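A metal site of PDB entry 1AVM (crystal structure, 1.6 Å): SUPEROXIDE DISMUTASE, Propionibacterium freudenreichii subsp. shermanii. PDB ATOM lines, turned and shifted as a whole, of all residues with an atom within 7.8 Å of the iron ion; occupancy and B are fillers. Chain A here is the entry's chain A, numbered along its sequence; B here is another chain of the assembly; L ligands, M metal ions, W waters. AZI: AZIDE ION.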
ATOM      1  N   HIS A  27      -1.400  -6.328 -24.170  1.00  0.00           N
ATOM      2  CA  HIS A  27      -0.060  -6.242 -24.703  1.00  0.00           C
ATOM      3  C   HIS A  27       0.236  -4.914 -25.404  1.00  0.00           C
ATOM      4  O   HIS A  27       1.283  -4.297 -25.169  1.00  0.00           O
ATOM      5  CB  HIS A  27       0.176  -7.405 -25.666  1.00  0.00           C
ATOM      6  CG  HIS A  27       1.621  -7.784 -25.825  1.00  0.00           C
ATOM      7  ND1 HIS A  27       2.024  -8.780 -26.674  1.00  0.00           N
ATOM      8  CD2 HIS A  27       2.732  -7.294 -25.244  1.00  0.00           C
ATOM      9  CE1 HIS A  27       3.341  -8.891 -26.622  1.00  0.00           C
ATOM     10  NE2 HIS A  27       3.794  -7.999 -25.751  1.00  0.00           N
ATOM     11  N   HIS A  28      -0.691  -4.467 -26.240  1.00  0.00           N
ATOM     12  CA  HIS A  28      -0.505  -3.231 -26.967  1.00  0.00           C
ATOM     13  C   HIS A  28      -0.874  -1.968 -26.177  1.00  0.00           C
ATOM     14  O   HIS A  28      -0.062  -1.051 -26.059  1.00  0.00           O
ATOM     15  CB  HIS A  28      -1.303  -3.273 -28.275  1.00  0.00           C
ATOM     16  CG  HIS A  28      -1.234  -2.002 -29.065  1.00  0.00           C
ATOM     17  ND1 HIS A  28      -2.091  -0.943 -28.848  1.00  0.00           N
ATOM     18  CD2 HIS A  28      -0.410  -1.607 -30.060  1.00  0.00           C
ATOM     19  CE1 HIS A  28      -1.799   0.048 -29.675  1.00  0.00           C
ATOM     20  NE2 HIS A  28      -0.784  -0.339 -30.420  1.00  0.00           N
ATOM     21  N   HIS A  31       1.188  -2.656 -21.982  1.00  0.00           N
ATOM     22  CA  HIS A  31       2.615  -2.921 -22.028  1.00  0.00           C
ATOM     23  C   HIS A  31       3.437  -2.072 -22.992  1.00  0.00           C
ATOM     24  O   HIS A  31       4.414  -1.440 -22.574  1.00  0.00           O
ATOM     25  CB  HIS A  31       2.890  -4.406 -22.267  1.00  0.00           C
ATOM     26  CG  HIS A  31       2.564  -5.273 -21.084  1.00  0.00           C
ATOM     27  ND1 HIS A  31       1.410  -6.016 -20.988  1.00  0.00           N
ATOM     28  CD2 HIS A  31       3.247  -5.501 -19.935  1.00  0.00           C
ATOM     29  CE1 HIS A  31       1.390  -6.652 -19.839  1.00  0.00           C
ATOM     30  NE2 HIS A  31       2.488  -6.357 -19.175  1.00  0.00           N
ATOM     31  N   HIS A  32       3.056  -2.043 -24.266  1.00  0.00           N
ATOM     32  CA  HIS A  32       3.799  -1.258 -25.251  1.00  0.00           C
ATOM     33  C   HIS A  32       3.759   0.231 -24.900  1.00  0.00           C
ATOM     34  O   HIS A  32       4.765   0.928 -25.017  1.00  0.00           O
ATOM     35  CB  HIS A  32       3.252  -1.507 -26.665  1.00  0.00           C
ATOM     36  CG  HIS A  32       4.145  -1.007 -27.760  1.00  0.00           C
ATOM     37  ND1 HIS A  32       3.912  -1.278 -29.088  1.00  0.00           N
ATOM     38  CD2 HIS A  32       5.270  -0.250 -27.726  1.00  0.00           C
ATOM     39  CE1 HIS A  32       4.848  -0.713 -29.829  1.00  0.00           C
ATOM     40  NE2 HIS A  32       5.689  -0.082 -29.026  1.00  0.00           N
ATOM     41  N   TYR A  35       6.419   1.302 -22.450  1.00  0.00           N
ATOM     42  CA  TYR A  35       7.757   1.414 -23.018  1.00  0.00           C
ATOM     43  C   TYR A  35       7.954   2.743 -23.750  1.00  0.00           C
ATOM     44  O   TYR A  35       9.031   3.330 -23.707  1.00  0.00           O
ATOM     45  CB  TYR A  35       8.057   0.245 -23.960  1.00  0.00           C
ATOM     46  CG  TYR A  35       8.032  -1.093 -23.270  1.00  0.00           C
ATOM     47  CD1 TYR A  35       8.625  -1.274 -22.023  1.00  0.00           C
ATOM     48  CD2 TYR A  35       7.380  -2.182 -23.850  1.00  0.00           C
ATOM     49  CE1 TYR A  35       8.572  -2.493 -21.366  1.00  0.00           C
ATOM     50  CE2 TYR A  35       7.323  -3.409 -23.204  1.00  0.00           C
ATOM     51  CZ  TYR A  35       7.919  -3.561 -21.968  1.00  0.00           C
ATOM     52  OH  TYR A  35       7.844  -4.772 -21.314  1.00  0.00           O
ATOM     53  N   GLY A  71      12.262  -2.057 -25.991  1.00  0.00           N
ATOM     54  CA  GLY A  71      10.923  -2.604 -25.855  1.00  0.00           C
ATOM     55  C   GLY A  71      10.001  -2.006 -26.904  1.00  0.00           C
ATOM     56  O   GLY A  71       9.176  -2.710 -27.484  1.00  0.00           O
ATOM     57  N   ASN A  74      11.146  -3.445 -30.458  1.00  0.00           N
ATOM     58  CA  ASN A  74      10.772  -4.844 -30.571  1.00  0.00           C
ATOM     59  C   ASN A  74       9.279  -5.045 -30.817  1.00  0.00           C
ATOM     60  O   ASN A  74       8.895  -5.853 -31.666  1.00  0.00           O
ATOM     61  CB  ASN A  74      11.205  -5.628 -29.330  1.00  0.00           C
ATOM     62  CG  ASN A  74      12.709  -5.735 -29.190  1.00  0.00           C
ATOM     63  OD1 ASN A  74      13.463  -5.354 -30.091  1.00  0.00           O
ATOM     64  ND2 ASN A  74      13.160  -6.259 -28.050  1.00  0.00           N
ATOM     65  N   HIS A  75       8.441  -4.342 -30.062  1.00  0.00           N
ATOM     66  CA  HIS A  75       7.005  -4.468 -30.221  1.00  0.00           C
ATOM     67  C   HIS A  75       6.479  -3.823 -31.500  1.00  0.00           C
ATOM     68  O   HIS A  75       5.546  -4.329 -32.102  1.00  0.00           O
ATOM     69  CB  HIS A  75       6.261  -3.954 -28.991  1.00  0.00           C
ATOM     70  CG  HIS A  75       6.426  -4.826 -27.792  1.00  0.00           C
ATOM     71  ND1 HIS A  75       7.444  -4.650 -26.879  1.00  0.00           N
ATOM     72  CD2 HIS A  75       5.738  -5.921 -27.392  1.00  0.00           C
ATOM     73  CE1 HIS A  75       7.377  -5.605 -25.965  1.00  0.00           C
ATOM     74  NE2 HIS A  75       6.358  -6.385 -26.248  1.00  0.00           N
ATOM     75  N   PHE A  78       7.117  -6.349 -33.971  1.00  0.00           N
ATOM     76  CA  PHE A  78       6.262  -7.483 -33.644  1.00  0.00           C
ATOM     77  C   PHE A  78       4.844  -7.392 -34.208  1.00  0.00           C
ATOM     78  O   PHE A  78       4.343  -8.349 -34.807  1.00  0.00           O
ATOM     79  CB  PHE A  78       6.228  -7.655 -32.111  1.00  0.00           C
ATOM     80  CG  PHE A  78       5.543  -8.909 -31.651  1.00  0.00           C
ATOM     81  CD1 PHE A  78       5.946 -10.157 -32.133  1.00  0.00           C
ATOM     82  CD2 PHE A  78       4.534  -8.846 -30.702  1.00  0.00           C
ATOM     83  CE1 PHE A  78       5.344 -11.319 -31.662  1.00  0.00           C
ATOM     84  CE2 PHE A  78       3.918 -10.011 -30.232  1.00  0.00           C
ATOM     85  CZ  PHE A  78       4.335 -11.256 -30.712  1.00  0.00           C
ATOM     86  N   TRP A  79       4.198  -6.237 -34.048  1.00  0.00           N
ATOM     87  CA  TRP A  79       2.824  -6.042 -34.520  1.00  0.00           C
ATOM     88  C   TRP A  79       2.729  -6.186 -36.039  1.00  0.00           C
ATOM     89  O   TRP A  79       1.825  -6.850 -36.549  1.00  0.00           O
ATOM     90  CB  TRP A  79       2.283  -4.673 -34.133  1.00  0.00           C
ATOM     91  CG  TRP A  79       2.367  -4.322 -32.685  1.00  0.00           C
ATOM     92  CD1 TRP A  79       2.743  -3.130 -32.154  1.00  0.00           C
ATOM     93  CD2 TRP A  79       2.066  -5.177 -31.565  1.00  0.00           C
ATOM     94  NE1 TRP A  79       2.700  -3.177 -30.782  1.00  0.00           N
ATOM     95  CE2 TRP A  79       2.278  -4.418 -30.392  1.00  0.00           C
ATOM     96  CE3 TRP A  79       1.628  -6.504 -31.445  1.00  0.00           C
ATOM     97  CZ2 TRP A  79       2.083  -4.947 -29.119  1.00  0.00           C
ATOM     98  CZ3 TRP A  79       1.423  -7.029 -30.163  1.00  0.00           C
ATOM     99  CH2 TRP A  79       1.654  -6.242 -29.016  1.00  0.00           C
ATOM    100  N   GLY A 125      12.587 -12.839 -22.943  1.00  0.00           N
ATOM    101  CA  GLY A 125      13.401 -12.642 -24.127  1.00  0.00           C
ATOM    102  C   GLY A 125      12.653 -12.680 -25.441  1.00  0.00           C
ATOM    103  O   GLY A 125      11.431 -12.731 -25.480  1.00  0.00           O
ATOM    104  N   TRP A 126      13.421 -12.627 -26.526  1.00  0.00           N
ATOM    105  CA  TRP A 126      12.875 -12.647 -27.877  1.00  0.00           C
ATOM    106  C   TRP A 126      13.675 -13.570 -28.784  1.00  0.00           C
ATOM    107  O   TRP A 126      14.871 -13.755 -28.603  1.00  0.00           O
ATOM    108  CB  TRP A 126      12.950 -11.251 -28.518  1.00  0.00           C
ATOM    109  CG  TRP A 126      12.148 -10.201 -27.849  1.00  0.00           C
ATOM    110  CD1 TRP A 126      12.404  -9.614 -26.643  1.00  0.00           C
ATOM    111  CD2 TRP A 126      10.945  -9.601 -28.341  1.00  0.00           C
ATOM    112  NE1 TRP A 126      11.437  -8.692 -26.349  1.00  0.00           N
ATOM    113  CE2 TRP A 126      10.520  -8.663 -27.371  1.00  0.00           C
ATOM    114  CE3 TRP A 126      10.169  -9.758 -29.499  1.00  0.00           C
ATOM    115  CZ2 TRP A 126       9.368  -7.889 -27.522  1.00  0.00           C
ATOM    116  CZ3 TRP A 126       9.019  -8.993 -29.654  1.00  0.00           C
ATOM    117  CH2 TRP A 126       8.638  -8.063 -28.671  1.00  0.00           C
ATOM    118  N   HIS A 146      14.856  -7.150 -23.460  1.00  0.00           N
ATOM    119  CA  HIS A 146      14.583  -6.469 -24.738  1.00  0.00           C
ATOM    120  C   HIS A 146      15.872  -5.985 -25.389  1.00  0.00           C
ATOM    121  O   HIS A 146      16.009  -6.005 -26.612  1.00  0.00           O
ATOM    122  CB  HIS A 146      13.726  -5.214 -24.535  1.00  0.00           C
ATOM    123  CG  HIS A 146      12.326  -5.479 -24.081  1.00  0.00           C
ATOM    124  ND1 HIS A 146      11.740  -4.791 -23.037  1.00  0.00           N
ATOM    125  CD2 HIS A 146      11.390  -6.344 -24.533  1.00  0.00           C
ATOM    126  CE1 HIS A 146      10.507  -5.222 -22.881  1.00  0.00           C
ATOM    127  NE2 HIS A 146      10.268  -6.167 -23.774  1.00  0.00           N
ATOM    128  N   ASP A 161       7.918 -12.396 -29.430  1.00  0.00           N
ATOM    129  CA  ASP A 161       7.949 -12.016 -28.024  1.00  0.00           C
ATOM    130  C   ASP A 161       7.780 -13.259 -27.145  1.00  0.00           C
ATOM    131  O   ASP A 161       6.725 -13.895 -27.164  1.00  0.00           O
ATOM    132  CB  ASP A 161       6.830 -11.016 -27.735  1.00  0.00           C
ATOM    133  CG  ASP A 161       6.967 -10.332 -26.378  1.00  0.00           C
ATOM    134  OD1 ASP A 161       7.866 -10.685 -25.593  1.00  0.00           O
ATOM    135  OD2 ASP A 161       6.160  -9.412 -26.099  1.00  0.00           O
ATOM    136  N   MET A 162       8.817 -13.599 -26.392  1.00  0.00           N
ATOM    137  CA  MET A 162       8.790 -14.757 -25.506  1.00  0.00           C
ATOM    138  C   MET A 162       8.626 -14.409 -24.030  1.00  0.00           C
ATOM    139  O   MET A 162       8.885 -15.240 -23.151  1.00  0.00           O
ATOM    140  CB  MET A 162       9.992 -15.657 -25.727  1.00  0.00           C
ATOM    141  CG  MET A 162       9.973 -16.397 -27.069  1.00  0.00           C
ATOM    142  SD  MET A 162       8.439 -17.319 -27.349  1.00  0.00           S
ATOM    143  CE  MET A 162       8.509 -18.537 -26.048  1.00  0.00           C
ATOM    144  N   TRP A 163       8.254 -13.155 -23.747  1.00  0.00           N
ATOM    145  CA  TRP A 163       7.999 -12.735 -22.378  1.00  0.00           C
ATOM    146  C   TRP A 163       6.705 -13.441 -22.012  1.00  0.00           C
ATOM    147  O   TRP A 163       5.843 -13.629 -22.867  1.00  0.00           O
ATOM    148  CB  TRP A 163       7.785 -11.220 -22.303  1.00  0.00           C
ATOM    149  CG  TRP A 163       9.030 -10.398 -22.302  1.00  0.00           C
ATOM    150  CD1 TRP A 163      10.040 -10.411 -23.214  1.00  0.00           C
ATOM    151  CD2 TRP A 163       9.389  -9.403 -21.332  1.00  0.00           C
ATOM    152  NE1 TRP A 163      10.992  -9.486 -22.890  1.00  0.00           N
ATOM    153  CE2 TRP A 163      10.629  -8.850 -21.736  1.00  0.00           C
ATOM    154  CE3 TRP A 163       8.773  -8.922 -20.163  1.00  0.00           C
ATOM    155  CZ2 TRP A 163      11.267  -7.842 -21.006  1.00  0.00           C
ATOM    156  CZ3 TRP A 163       9.418  -7.910 -19.439  1.00  0.00           C
ATOM    157  CH2 TRP A 163      10.650  -7.381 -19.869  1.00  0.00           C
ATOM    158  N   GLU A 164       6.552 -13.843 -20.752  1.00  0.00           N
ATOM    159  CA  GLU A 164       5.354 -14.553 -20.325  1.00  0.00           C
ATOM    160  C   GLU A 164       4.021 -13.846 -20.569  1.00  0.00           C
ATOM    161  O   GLU A 164       3.022 -14.502 -20.844  1.00  0.00           O
ATOM    162  CB  GLU A 164       5.501 -14.994 -18.872  1.00  0.00           C
ATOM    163  CG  GLU A 164       6.645 -16.005 -18.694  1.00  0.00           C
ATOM    164  CD  GLU A 164       6.932 -16.372 -17.261  1.00  0.00           C
ATOM    165  OE1 GLU A 164       6.858 -15.495 -16.377  1.00  0.00           O
ATOM    166  OE2 GLU A 164       7.262 -17.548 -17.007  1.00  0.00           O
ATOM    167  N   HIS A 165       4.013 -12.521 -20.538  1.00  0.00           N
ATOM    168  CA  HIS A 165       2.770 -11.764 -20.775  1.00  0.00           C
ATOM    169  C   HIS A 165       2.253 -11.934 -22.200  1.00  0.00           C
ATOM    170  O   HIS A 165       1.086 -11.667 -22.476  1.00  0.00           O
ATOM    171  CB  HIS A 165       2.971 -10.265 -20.472  1.00  0.00           C
ATOM    172  CG  HIS A 165       3.937  -9.577 -21.399  1.00  0.00           C
ATOM    173  ND1 HIS A 165       5.105  -9.013 -20.955  1.00  0.00           N
ATOM    174  CD2 HIS A 165       3.882  -9.336 -22.731  1.00  0.00           C
ATOM    175  CE1 HIS A 165       5.743  -8.461 -21.974  1.00  0.00           C
ATOM    176  NE2 HIS A 165       5.022  -8.637 -23.063  1.00  0.00           N
ATOM    177  N   ALA A 166       3.138 -12.362 -23.096  1.00  0.00           N
ATOM    178  CA  ALA A 166       2.779 -12.542 -24.493  1.00  0.00           C
ATOM    179  C   ALA A 166       1.991 -13.819 -24.771  1.00  0.00           C
ATOM    180  O   ALA A 166       1.332 -13.926 -25.805  1.00  0.00           O
ATOM    181  CB  ALA A 166       4.022 -12.507 -25.367  1.00  0.00           C
ATOM    182  N   TYR A 178       2.376 -22.058 -28.022  1.00  0.00           N
ATOM    183  CA  TYR A 178       2.342 -20.657 -28.429  1.00  0.00           C
ATOM    184  C   TYR A 178       3.152 -20.433 -29.701  1.00  0.00           C
ATOM    185  O   TYR A 178       2.666 -19.784 -30.639  1.00  0.00           O
ATOM    186  CB  TYR A 178       2.874 -19.772 -27.298  1.00  0.00           C
ATOM    187  CG  TYR A 178       3.224 -18.350 -27.678  1.00  0.00           C
ATOM    188  CD1 TYR A 178       2.272 -17.487 -28.230  1.00  0.00           C
ATOM    189  CD2 TYR A 178       4.492 -17.844 -27.430  1.00  0.00           C
ATOM    190  CE1 TYR A 178       2.581 -16.159 -28.521  1.00  0.00           C
ATOM    191  CE2 TYR A 178       4.815 -16.519 -27.706  1.00  0.00           C
ATOM    192  CZ  TYR A 178       3.853 -15.682 -28.254  1.00  0.00           C
ATOM    193  OH  TYR A 178       4.174 -14.366 -28.488  1.00  0.00           O
ATOM    194  N   GLU B 164       6.353 -12.771 -14.360  1.00  0.00           N
ATOM    195  CA  GLU B 164       4.959 -12.652 -14.773  1.00  0.00           C
ATOM    196  C   GLU B 164       4.075 -13.862 -14.518  1.00  0.00           C
ATOM    197  O   GLU B 164       2.907 -13.703 -14.170  1.00  0.00           O
ATOM    198  CB  GLU B 164       4.880 -12.183 -16.228  1.00  0.00           C
ATOM    199  CG  GLU B 164       5.368 -10.748 -16.416  1.00  0.00           C
ATOM    200  CD  GLU B 164       5.492 -10.323 -17.867  1.00  0.00           C
ATOM    201  OE1 GLU B 164       5.807 -11.158 -18.722  1.00  0.00           O
ATOM    202  OE2 GLU B 164       5.288  -9.121 -18.139  1.00  0.00           O
HETATM  203  N1  AZI L   1       5.365  -6.144 -23.695  1.00  0.00           N
HETATM  204  N2  AZI L   1       4.995  -5.139 -24.342  1.00  0.00           N
HETATM  205  N3  AZI L   1       4.672  -4.269 -24.910  1.00  0.00           N
HETATM  206 FE    FE M   1       5.802  -7.968 -24.927  1.00  0.00          FE
HETATM  207  O   HOH W   1       7.824  -8.074 -24.218  1.00  0.00           O
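Water W1 bridges OD1 of Asp 161 (3.0 Å) and NE2 of His 146 (3.1 Å).
The iron ion is bound by the side-chain carboxylate (OD2) of Asp 161 (1.9 Å), a ring nitrogen (NE2) of His 165 (2.1 Å), a ring nitrogen (NE2) of His 75 (2.1 Å), water W1 (2.1 Å), a ring nitrogen (NE2) of His 27 (2.2 Å) and a nitrogen (N1) of the ligand (2.2 Å).
The iron ion has six donor atoms within binding distance.
The nearest printed residue that does not touch the iron ion is Trp 126 (4.4 Å).
The backbone carbonyl oxygen (O) of Gly 71 lies within hydrogen-bond range of a ring nitrogen (ND1) of His 75 (2.7 Å).
O of His 75 lies close to NE1 of Trp 79, 3.3 Å away.
The backbone carbonyl oxygen of His 27 lies within hydrogen-bond range of the backbone NH of His 32 (3.0 Å).
OE2 of Glu 164 of chain B is in hydrogen-bond range of ND1 of His 165 (2.8 Å).
The backbone carbonyl oxygen (O) of Asp 161 lies within hydrogen-bond range of the side-chain hydroxyl (OH) of Tyr 178, 2.9 Å away.
OD1 of Asp 161 sits at hydrogen-bond distance from N of Trp 163.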
